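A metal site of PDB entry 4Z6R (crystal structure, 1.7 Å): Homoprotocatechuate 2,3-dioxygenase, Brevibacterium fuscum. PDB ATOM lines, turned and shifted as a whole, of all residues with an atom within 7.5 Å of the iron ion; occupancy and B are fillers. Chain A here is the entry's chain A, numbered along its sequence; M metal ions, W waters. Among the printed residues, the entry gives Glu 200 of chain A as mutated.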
ATOM      1  N   ASP A 154      35.793 -30.326 -24.654  1.00  0.00           N
ATOM      2  CA  ASP A 154      35.077 -31.502 -24.314  1.00  0.00           C
ATOM      3  C   ASP A 154      33.636 -31.541 -24.855  1.00  0.00           C
ATOM      4  O   ASP A 154      33.241 -32.578 -25.450  1.00  0.00           O
ATOM      5  CB  ASP A 154      35.032 -31.795 -22.826  1.00  0.00           C
ATOM      6  CG  ASP A 154      34.522 -33.226 -22.558  1.00  0.00           C
ATOM      7  OD1 ASP A 154      35.313 -34.162 -22.843  1.00  0.00           O
ATOM      8  OD2 ASP A 154      33.331 -33.431 -22.215  1.00  0.00           O
ATOM      9  N   HIS A 155      32.834 -30.517 -24.573  1.00  0.00           N
ATOM     10  CA  HIS A 155      31.390 -30.550 -24.935  1.00  0.00           C
ATOM     11  C   HIS A 155      30.686 -29.216 -24.891  1.00  0.00           C
ATOM     12  O   HIS A 155      31.201 -28.251 -24.368  1.00  0.00           O
ATOM     13  CB  HIS A 155      30.648 -31.544 -24.002  1.00  0.00           C
ATOM     14  CG  HIS A 155      30.561 -31.110 -22.564  1.00  0.00           C
ATOM     15  ND1 HIS A 155      31.455 -31.540 -21.607  1.00  0.00           N
ATOM     16  CD2 HIS A 155      29.644 -30.347 -21.911  1.00  0.00           C
ATOM     17  CE1 HIS A 155      31.115 -31.035 -20.422  1.00  0.00           C
ATOM     18  NE2 HIS A 155      30.016 -30.323 -20.580  1.00  0.00           N
ATOM     19  N   PHE A 156      29.475 -29.203 -25.408  1.00  0.00           N
ATOM     20  CA  PHE A 156      28.534 -28.112 -25.308  1.00  0.00           C
ATOM     21  C   PHE A 156      27.374 -28.559 -24.431  1.00  0.00           C
ATOM     22  O   PHE A 156      27.088 -29.750 -24.292  1.00  0.00           O
ATOM     23  CB  PHE A 156      27.960 -27.757 -26.696  1.00  0.00           C
ATOM     24  CG  PHE A 156      28.983 -27.595 -27.808  1.00  0.00           C
ATOM     25  CD1 PHE A 156      29.990 -26.632 -27.736  1.00  0.00           C
ATOM     26  CD2 PHE A 156      28.893 -28.362 -28.957  1.00  0.00           C
ATOM     27  CE1 PHE A 156      30.894 -26.471 -28.754  1.00  0.00           C
ATOM     28  CE2 PHE A 156      29.795 -28.197 -29.992  1.00  0.00           C
ATOM     29  CZ  PHE A 156      30.792 -27.248 -29.892  1.00  0.00           C
ATOM     30  N   ASN A 157      26.632 -27.612 -23.890  1.00  0.00           N
ATOM     31  CA  ASN A 157      25.386 -27.989 -23.222  1.00  0.00           C
ATOM     32  C   ASN A 157      24.342 -26.968 -23.581  1.00  0.00           C
ATOM     33  O   ASN A 157      24.621 -25.809 -23.442  1.00  0.00           O
ATOM     34  CB  ASN A 157      25.627 -28.011 -21.692  1.00  0.00           C
ATOM     35  CG  ASN A 157      24.420 -28.451 -20.915  1.00  0.00           C
ATOM     36  OD1 ASN A 157      23.385 -27.866 -21.048  1.00  0.00           O
ATOM     37  ND2 ASN A 157      24.562 -29.470 -20.106  1.00  0.00           N
ATOM     38  N   TRP A 192      22.355 -36.390 -21.417  1.00  0.00           N
ATOM     39  CA  TRP A 192      23.709 -36.280 -21.980  1.00  0.00           C
ATOM     40  C   TRP A 192      23.916 -37.269 -23.105  1.00  0.00           C
ATOM     41  O   TRP A 192      23.505 -38.412 -22.991  1.00  0.00           O
ATOM     42  CB  TRP A 192      24.705 -36.574 -20.855  1.00  0.00           C
ATOM     43  CG  TRP A 192      24.825 -35.452 -19.821  1.00  0.00           C
ATOM     44  CD1 TRP A 192      25.864 -34.576 -19.671  1.00  0.00           C
ATOM     45  CD2 TRP A 192      23.864 -35.101 -18.804  1.00  0.00           C
ATOM     46  NE1 TRP A 192      25.617 -33.695 -18.619  1.00  0.00           N
ATOM     47  CE2 TRP A 192      24.401 -33.984 -18.083  1.00  0.00           C
ATOM     48  CE3 TRP A 192      22.624 -35.620 -18.416  1.00  0.00           C
ATOM     49  CZ2 TRP A 192      23.741 -33.399 -16.971  1.00  0.00           C
ATOM     50  CZ3 TRP A 192      21.933 -35.001 -17.326  1.00  0.00           C
ATOM     51  CH2 TRP A 192      22.524 -33.910 -16.621  1.00  0.00           C
ATOM     52  N   GLU A 200      29.793 -37.071 -23.027  1.00  0.00           N
ATOM     53  CA  GLU A 200      29.040 -36.045 -23.758  1.00  0.00           C
ATOM     54  C   GLU A 200      29.846 -35.359 -24.846  1.00  0.00           C
ATOM     55  O   GLU A 200      31.019 -34.998 -24.629  1.00  0.00           O
ATOM     56  CB  GLU A 200      28.502 -34.971 -22.801  1.00  0.00           C
ATOM     57  CG  GLU A 200      29.409 -34.658 -21.644  1.00  0.00           C
ATOM     58  CD  GLU A 200      28.838 -33.633 -20.665  1.00  0.00           C
ATOM     59  OE1 GLU A 200      27.991 -32.767 -21.085  1.00  0.00           O
ATOM     60  OE2 GLU A 200      29.250 -33.719 -19.476  1.00  0.00           O
ATOM     61  N   ALA A 203      24.700 -31.859 -24.704  1.00  0.00           N
ATOM     62  CA  ALA A 203      23.838 -32.246 -23.600  1.00  0.00           C
ATOM     63  C   ALA A 203      22.674 -31.305 -23.657  1.00  0.00           C
ATOM     64  O   ALA A 203      22.778 -30.172 -24.140  1.00  0.00           O
ATOM     65  CB  ALA A 203      24.572 -32.136 -22.276  1.00  0.00           C
ATOM     66  N   HIS A 213      23.908 -23.245 -22.622  1.00  0.00           N
ATOM     67  CA  HIS A 213      24.211 -23.289 -21.219  1.00  0.00           C
ATOM     68  C   HIS A 213      25.713 -23.039 -20.945  1.00  0.00           C
ATOM     69  O   HIS A 213      26.052 -22.146 -20.193  1.00  0.00           O
ATOM     70  CB  HIS A 213      23.751 -24.566 -20.563  1.00  0.00           C
ATOM     71  CG  HIS A 213      23.686 -24.432 -19.094  1.00  0.00           C
ATOM     72  ND1 HIS A 213      24.802 -24.521 -18.296  1.00  0.00           N
ATOM     73  CD2 HIS A 213      22.666 -24.077 -18.278  1.00  0.00           C
ATOM     74  CE1 HIS A 213      24.458 -24.289 -17.030  1.00  0.00           C
ATOM     75  NE2 HIS A 213      23.165 -24.020 -17.003  1.00  0.00           N
ATOM     76  N   HIS A 214      26.577 -23.840 -21.569  1.00  0.00           N
ATOM     77  CA  HIS A 214      28.006 -23.609 -21.447  1.00  0.00           C
ATOM     78  C   HIS A 214      28.752 -24.339 -22.524  1.00  0.00           C
ATOM     79  O   HIS A 214      28.196 -25.193 -23.221  1.00  0.00           O
ATOM     80  CB  HIS A 214      28.505 -24.060 -20.055  1.00  0.00           C
ATOM     81  CG  HIS A 214      28.246 -25.507 -19.751  1.00  0.00           C
ATOM     82  ND1 HIS A 214      27.137 -25.940 -19.068  1.00  0.00           N
ATOM     83  CD2 HIS A 214      28.985 -26.613 -20.003  1.00  0.00           C
ATOM     84  CE1 HIS A 214      27.185 -27.246 -18.922  1.00  0.00           C
ATOM     85  NE2 HIS A 214      28.308 -27.673 -19.478  1.00  0.00           N
ATOM     86  N   VAL A 215      30.030 -23.982 -22.630  1.00  0.00           N
ATOM     87  CA  VAL A 215      31.012 -24.724 -23.368  1.00  0.00           C
ATOM     88  C   VAL A 215      31.989 -25.292 -22.355  1.00  0.00           C
ATOM     89  O   VAL A 215      32.326 -24.604 -21.406  1.00  0.00           O
ATOM     90  CB  VAL A 215      31.752 -23.750 -24.337  1.00  0.00           C
ATOM     91  CG1 VAL A 215      32.962 -24.436 -24.909  1.00  0.00           C
ATOM     92  CG2 VAL A 215      30.783 -23.304 -25.435  1.00  0.00           C
ATOM     93  N   ALA A 216      32.480 -26.520 -22.556  1.00  0.00           N
ATOM     94  CA  ALA A 216      33.360 -27.177 -21.540  1.00  0.00           C
ATOM     95  C   ALA A 216      34.726 -27.541 -22.083  1.00  0.00           C
ATOM     96  O   ALA A 216      34.841 -28.148 -23.174  1.00  0.00           O
ATOM     97  CB  ALA A 216      32.674 -28.436 -20.980  1.00  0.00           C
ATOM     98  N   HIS A 248      30.797 -34.059 -10.096  1.00  0.00           N
ATOM     99  CA  HIS A 248      29.454 -34.329 -10.666  1.00  0.00           C
ATOM    100  C   HIS A 248      28.973 -35.723 -10.210  1.00  0.00           C
ATOM    101  O   HIS A 248      29.784 -36.683 -10.073  1.00  0.00           O
ATOM    102  CB  HIS A 248      29.479 -34.292 -12.201  1.00  0.00           C
ATOM    103  CG  HIS A 248      29.451 -32.909 -12.796  1.00  0.00           C
ATOM    104  ND1 HIS A 248      28.553 -31.932 -12.402  1.00  0.00           N
ATOM    105  CD2 HIS A 248      30.156 -32.371 -13.818  1.00  0.00           C
ATOM    106  CE1 HIS A 248      28.731 -30.854 -13.133  1.00  0.00           C
ATOM    107  NE2 HIS A 248      29.706 -31.084 -13.990  1.00  0.00           N
ATOM    108  N   SER A 251      28.020 -37.954 -15.024  1.00  0.00           N
ATOM    109  CA  SER A 251      29.348 -37.862 -15.685  1.00  0.00           C
ATOM    110  C   SER A 251      30.497 -38.287 -14.789  1.00  0.00           C
ATOM    111  O   SER A 251      31.544 -38.686 -15.299  1.00  0.00           O
ATOM    112  CB  SER A 251      29.677 -36.502 -16.289  1.00  0.00           C
ATOM    113  OG  SER A 251      30.162 -35.588 -15.336  1.00  0.00           O
ATOM    114  N   TYR A 255      34.678 -30.751 -11.730  1.00  0.00           N
ATOM    115  CA  TYR A 255      34.147 -29.624 -12.489  1.00  0.00           C
ATOM    116  C   TYR A 255      34.242 -28.287 -11.798  1.00  0.00           C
ATOM    117  O   TYR A 255      34.391 -28.170 -10.560  1.00  0.00           O
ATOM    118  CB  TYR A 255      32.688 -29.895 -12.874  1.00  0.00           C
ATOM    119  CG  TYR A 255      31.730 -29.708 -11.722  1.00  0.00           C
ATOM    120  CD1 TYR A 255      31.247 -28.461 -11.407  1.00  0.00           C
ATOM    121  CD2 TYR A 255      31.359 -30.786 -10.908  1.00  0.00           C
ATOM    122  CE1 TYR A 255      30.360 -28.266 -10.344  1.00  0.00           C
ATOM    123  CE2 TYR A 255      30.513 -30.590  -9.816  1.00  0.00           C
ATOM    124  CZ  TYR A 255      29.993 -29.345  -9.543  1.00  0.00           C
ATOM    125  OH  TYR A 255      29.126 -29.143  -8.451  1.00  0.00           O
ATOM    126  N   TYR A 257      32.417 -24.202 -12.747  1.00  0.00           N
ATOM    127  CA  TYR A 257      31.717 -23.250 -13.679  1.00  0.00           C
ATOM    128  C   TYR A 257      32.126 -21.802 -13.413  1.00  0.00           C
ATOM    129  O   TYR A 257      32.024 -21.301 -12.264  1.00  0.00           O
ATOM    130  CB  TYR A 257      30.185 -23.353 -13.608  1.00  0.00           C
ATOM    131  CG  TYR A 257      29.618 -24.730 -14.003  1.00  0.00           C
ATOM    132  CD1 TYR A 257      29.359 -25.063 -15.315  1.00  0.00           C
ATOM    133  CD2 TYR A 257      29.405 -25.702 -13.022  1.00  0.00           C
ATOM    134  CE1 TYR A 257      28.871 -26.311 -15.663  1.00  0.00           C
ATOM    135  CE2 TYR A 257      28.897 -26.973 -13.360  1.00  0.00           C
ATOM    136  CZ  TYR A 257      28.640 -27.265 -14.667  1.00  0.00           C
ATOM    137  OH  TYR A 257      28.154 -28.521 -14.968  1.00  0.00           O
ATOM    138  N   GLU A 267      32.571 -24.301 -18.540  1.00  0.00           N
ATOM    139  CA  GLU A 267      32.884 -25.344 -17.579  1.00  0.00           C
ATOM    140  C   GLU A 267      34.302 -25.819 -17.780  1.00  0.00           C
ATOM    141  O   GLU A 267      34.771 -25.967 -18.933  1.00  0.00           O
ATOM    142  CB  GLU A 267      31.910 -26.534 -17.735  1.00  0.00           C
ATOM    143  CG  GLU A 267      32.139 -27.616 -16.709  1.00  0.00           C
ATOM    144  CD  GLU A 267      31.205 -28.795 -16.844  1.00  0.00           C
ATOM    145  OE1 GLU A 267      30.629 -28.934 -17.929  1.00  0.00           O
ATOM    146  OE2 GLU A 267      31.046 -29.554 -15.853  1.00  0.00           O
ATOM    147  N   ILE A 268      35.000 -26.065 -16.680  1.00  0.00           N
ATOM    148  CA  ILE A 268      36.217 -26.833 -16.687  1.00  0.00           C
ATOM    149  C   ILE A 268      35.958 -28.207 -16.087  1.00  0.00           C
ATOM    150  O   ILE A 268      35.254 -28.292 -15.057  1.00  0.00           O
ATOM    151  CB  ILE A 268      37.328 -26.145 -15.871  1.00  0.00           C
ATOM    152  CG1 ILE A 268      37.290 -24.599 -15.980  1.00  0.00           C
ATOM    153  CG2 ILE A 268      38.701 -26.635 -16.312  1.00  0.00           C
ATOM    154  CD1 ILE A 268      37.472 -24.105 -17.362  1.00  0.00           C
ATOM    155  N   TYR A 269      36.496 -29.252 -16.701  1.00  0.00           N
ATOM    156  CA  TYR A 269      35.976 -30.614 -16.540  1.00  0.00           C
ATOM    157  C   TYR A 269      37.137 -31.576 -16.610  1.00  0.00           C
ATOM    158  O   TYR A 269      38.031 -31.402 -17.453  1.00  0.00           O
ATOM    159  CB  TYR A 269      35.006 -30.828 -17.712  1.00  0.00           C
ATOM    160  CG  TYR A 269      34.224 -32.048 -17.873  1.00  0.00           C
ATOM    161  CD1 TYR A 269      32.930 -32.100 -17.383  1.00  0.00           C
ATOM    162  CD2 TYR A 269      34.670 -33.085 -18.669  1.00  0.00           C
ATOM    163  CE1 TYR A 269      32.149 -33.198 -17.606  1.00  0.00           C
ATOM    164  CE2 TYR A 269      33.870 -34.185 -18.951  1.00  0.00           C
ATOM    165  CZ  TYR A 269      32.595 -34.234 -18.402  1.00  0.00           C
ATOM    166  OH  TYR A 269      31.721 -35.283 -18.632  1.00  0.00           O
ATOM    167  N   TRP A 304      22.570 -20.895 -12.016  1.00  0.00           N
ATOM    168  CA  TRP A 304      22.966 -21.999 -12.877  1.00  0.00           C
ATOM    169  C   TRP A 304      21.769 -22.548 -13.644  1.00  0.00           C
ATOM    170  O   TRP A 304      21.878 -22.981 -14.811  1.00  0.00           O
ATOM    171  CB  TRP A 304      23.614 -23.101 -12.034  1.00  0.00           C
ATOM    172  CG  TRP A 304      24.406 -24.074 -12.842  1.00  0.00           C
ATOM    173  CD1 TRP A 304      25.721 -23.952 -13.157  1.00  0.00           C
ATOM    174  CD2 TRP A 304      23.935 -25.244 -13.469  1.00  0.00           C
ATOM    175  NE1 TRP A 304      26.095 -24.981 -13.957  1.00  0.00           N
ATOM    176  CE2 TRP A 304      25.024 -25.811 -14.138  1.00  0.00           C
ATOM    177  CE3 TRP A 304      22.720 -25.903 -13.496  1.00  0.00           C
ATOM    178  CZ2 TRP A 304      24.930 -26.977 -14.865  1.00  0.00           C
ATOM    179  CZ3 TRP A 304      22.625 -27.057 -14.232  1.00  0.00           C
ATOM    180  CH2 TRP A 304      23.741 -27.581 -14.918  1.00  0.00           C
HETATM  181 FE    FE M   1      28.866 -29.769 -18.729  1.00  0.00          FE
HETATM  182  O   HOH W   1      27.022 -30.755 -19.582  1.00  0.00           O
HETATM  183  O   HOH W   2      27.847 -29.821 -17.038  1.00  0.00           O
HETATM  184  O   HOH W   3      29.120 -31.764 -17.666  1.00  0.00           O
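The side-chain hydroxyl (OH) of Tyr 257 is in hydrogen-bond range of the side-chain carboxylate (OE2) of Glu 267, at 3.2 Å. O of Val 215 sits at hydrogen-bond distance from N of Glu 267, 2.9 Å away. NE2 of His 155 lies close to OE1 of Glu 200, 3.2 Å away. The backbone NH (N) of Ala 216 sits at hydrogen-bond distance from the backbone carbonyl oxygen (O) of His 155 (2.8 Å). The side-chain carboxylate (OD2) of Asp 154 is in hydrogen-bond range of a ring nitrogen (ND1) of His 155 (2.7 Å). The backbone carbonyl oxygen of His 214 is in hydrogen-bond range of the backbone NH of Asn 157. ND1 of His 214 sits at hydrogen-bond distance from ND1 of His 213, 2.8 Å away. OE2 of Glu 200 is in hydrogen-bond range of OH of Tyr 269 (3.0 Å).
Glu 200 touches the iron ion (OE1 to FE, 3.9 Å). Within 4 Å of the iron ion: His 155, Glu 200, His 214 and Glu 267. The nearest printed residue that does not touch the iron ion is Tyr 257 (4.03 Å).
Water W2 binds the iron ion (2.0 Å). The iron ion is bound by OE1 of Glu 267 (2.1 Å). A ring nitrogen (NE2) of His 155 binds the iron ion, 2.2 Å away. Water W1 binds the iron ion, 2.3 Å away. Water W3 binds the iron ion. NE2 of His 214 binds the iron ion, at 2.3 Å. The iron ion has six donor atoms within binding distance.
Water W1 lies within hydrogen-bond range of OE1 of Glu 200 (2.7 Å), ND2 of Asn 157 (2.8 Å) and NE1 of Trp 192 (3.4 Å). Water W2 lies within hydrogen-bond range of OH of Tyr 257 and OE2 of Glu 267. Water W3 bridges the side-chain carboxylate (OE2) of Glu 200 (2.7 Å) and the side-chain carboxylate (OE2) of Glu 267 (3.4 Å).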
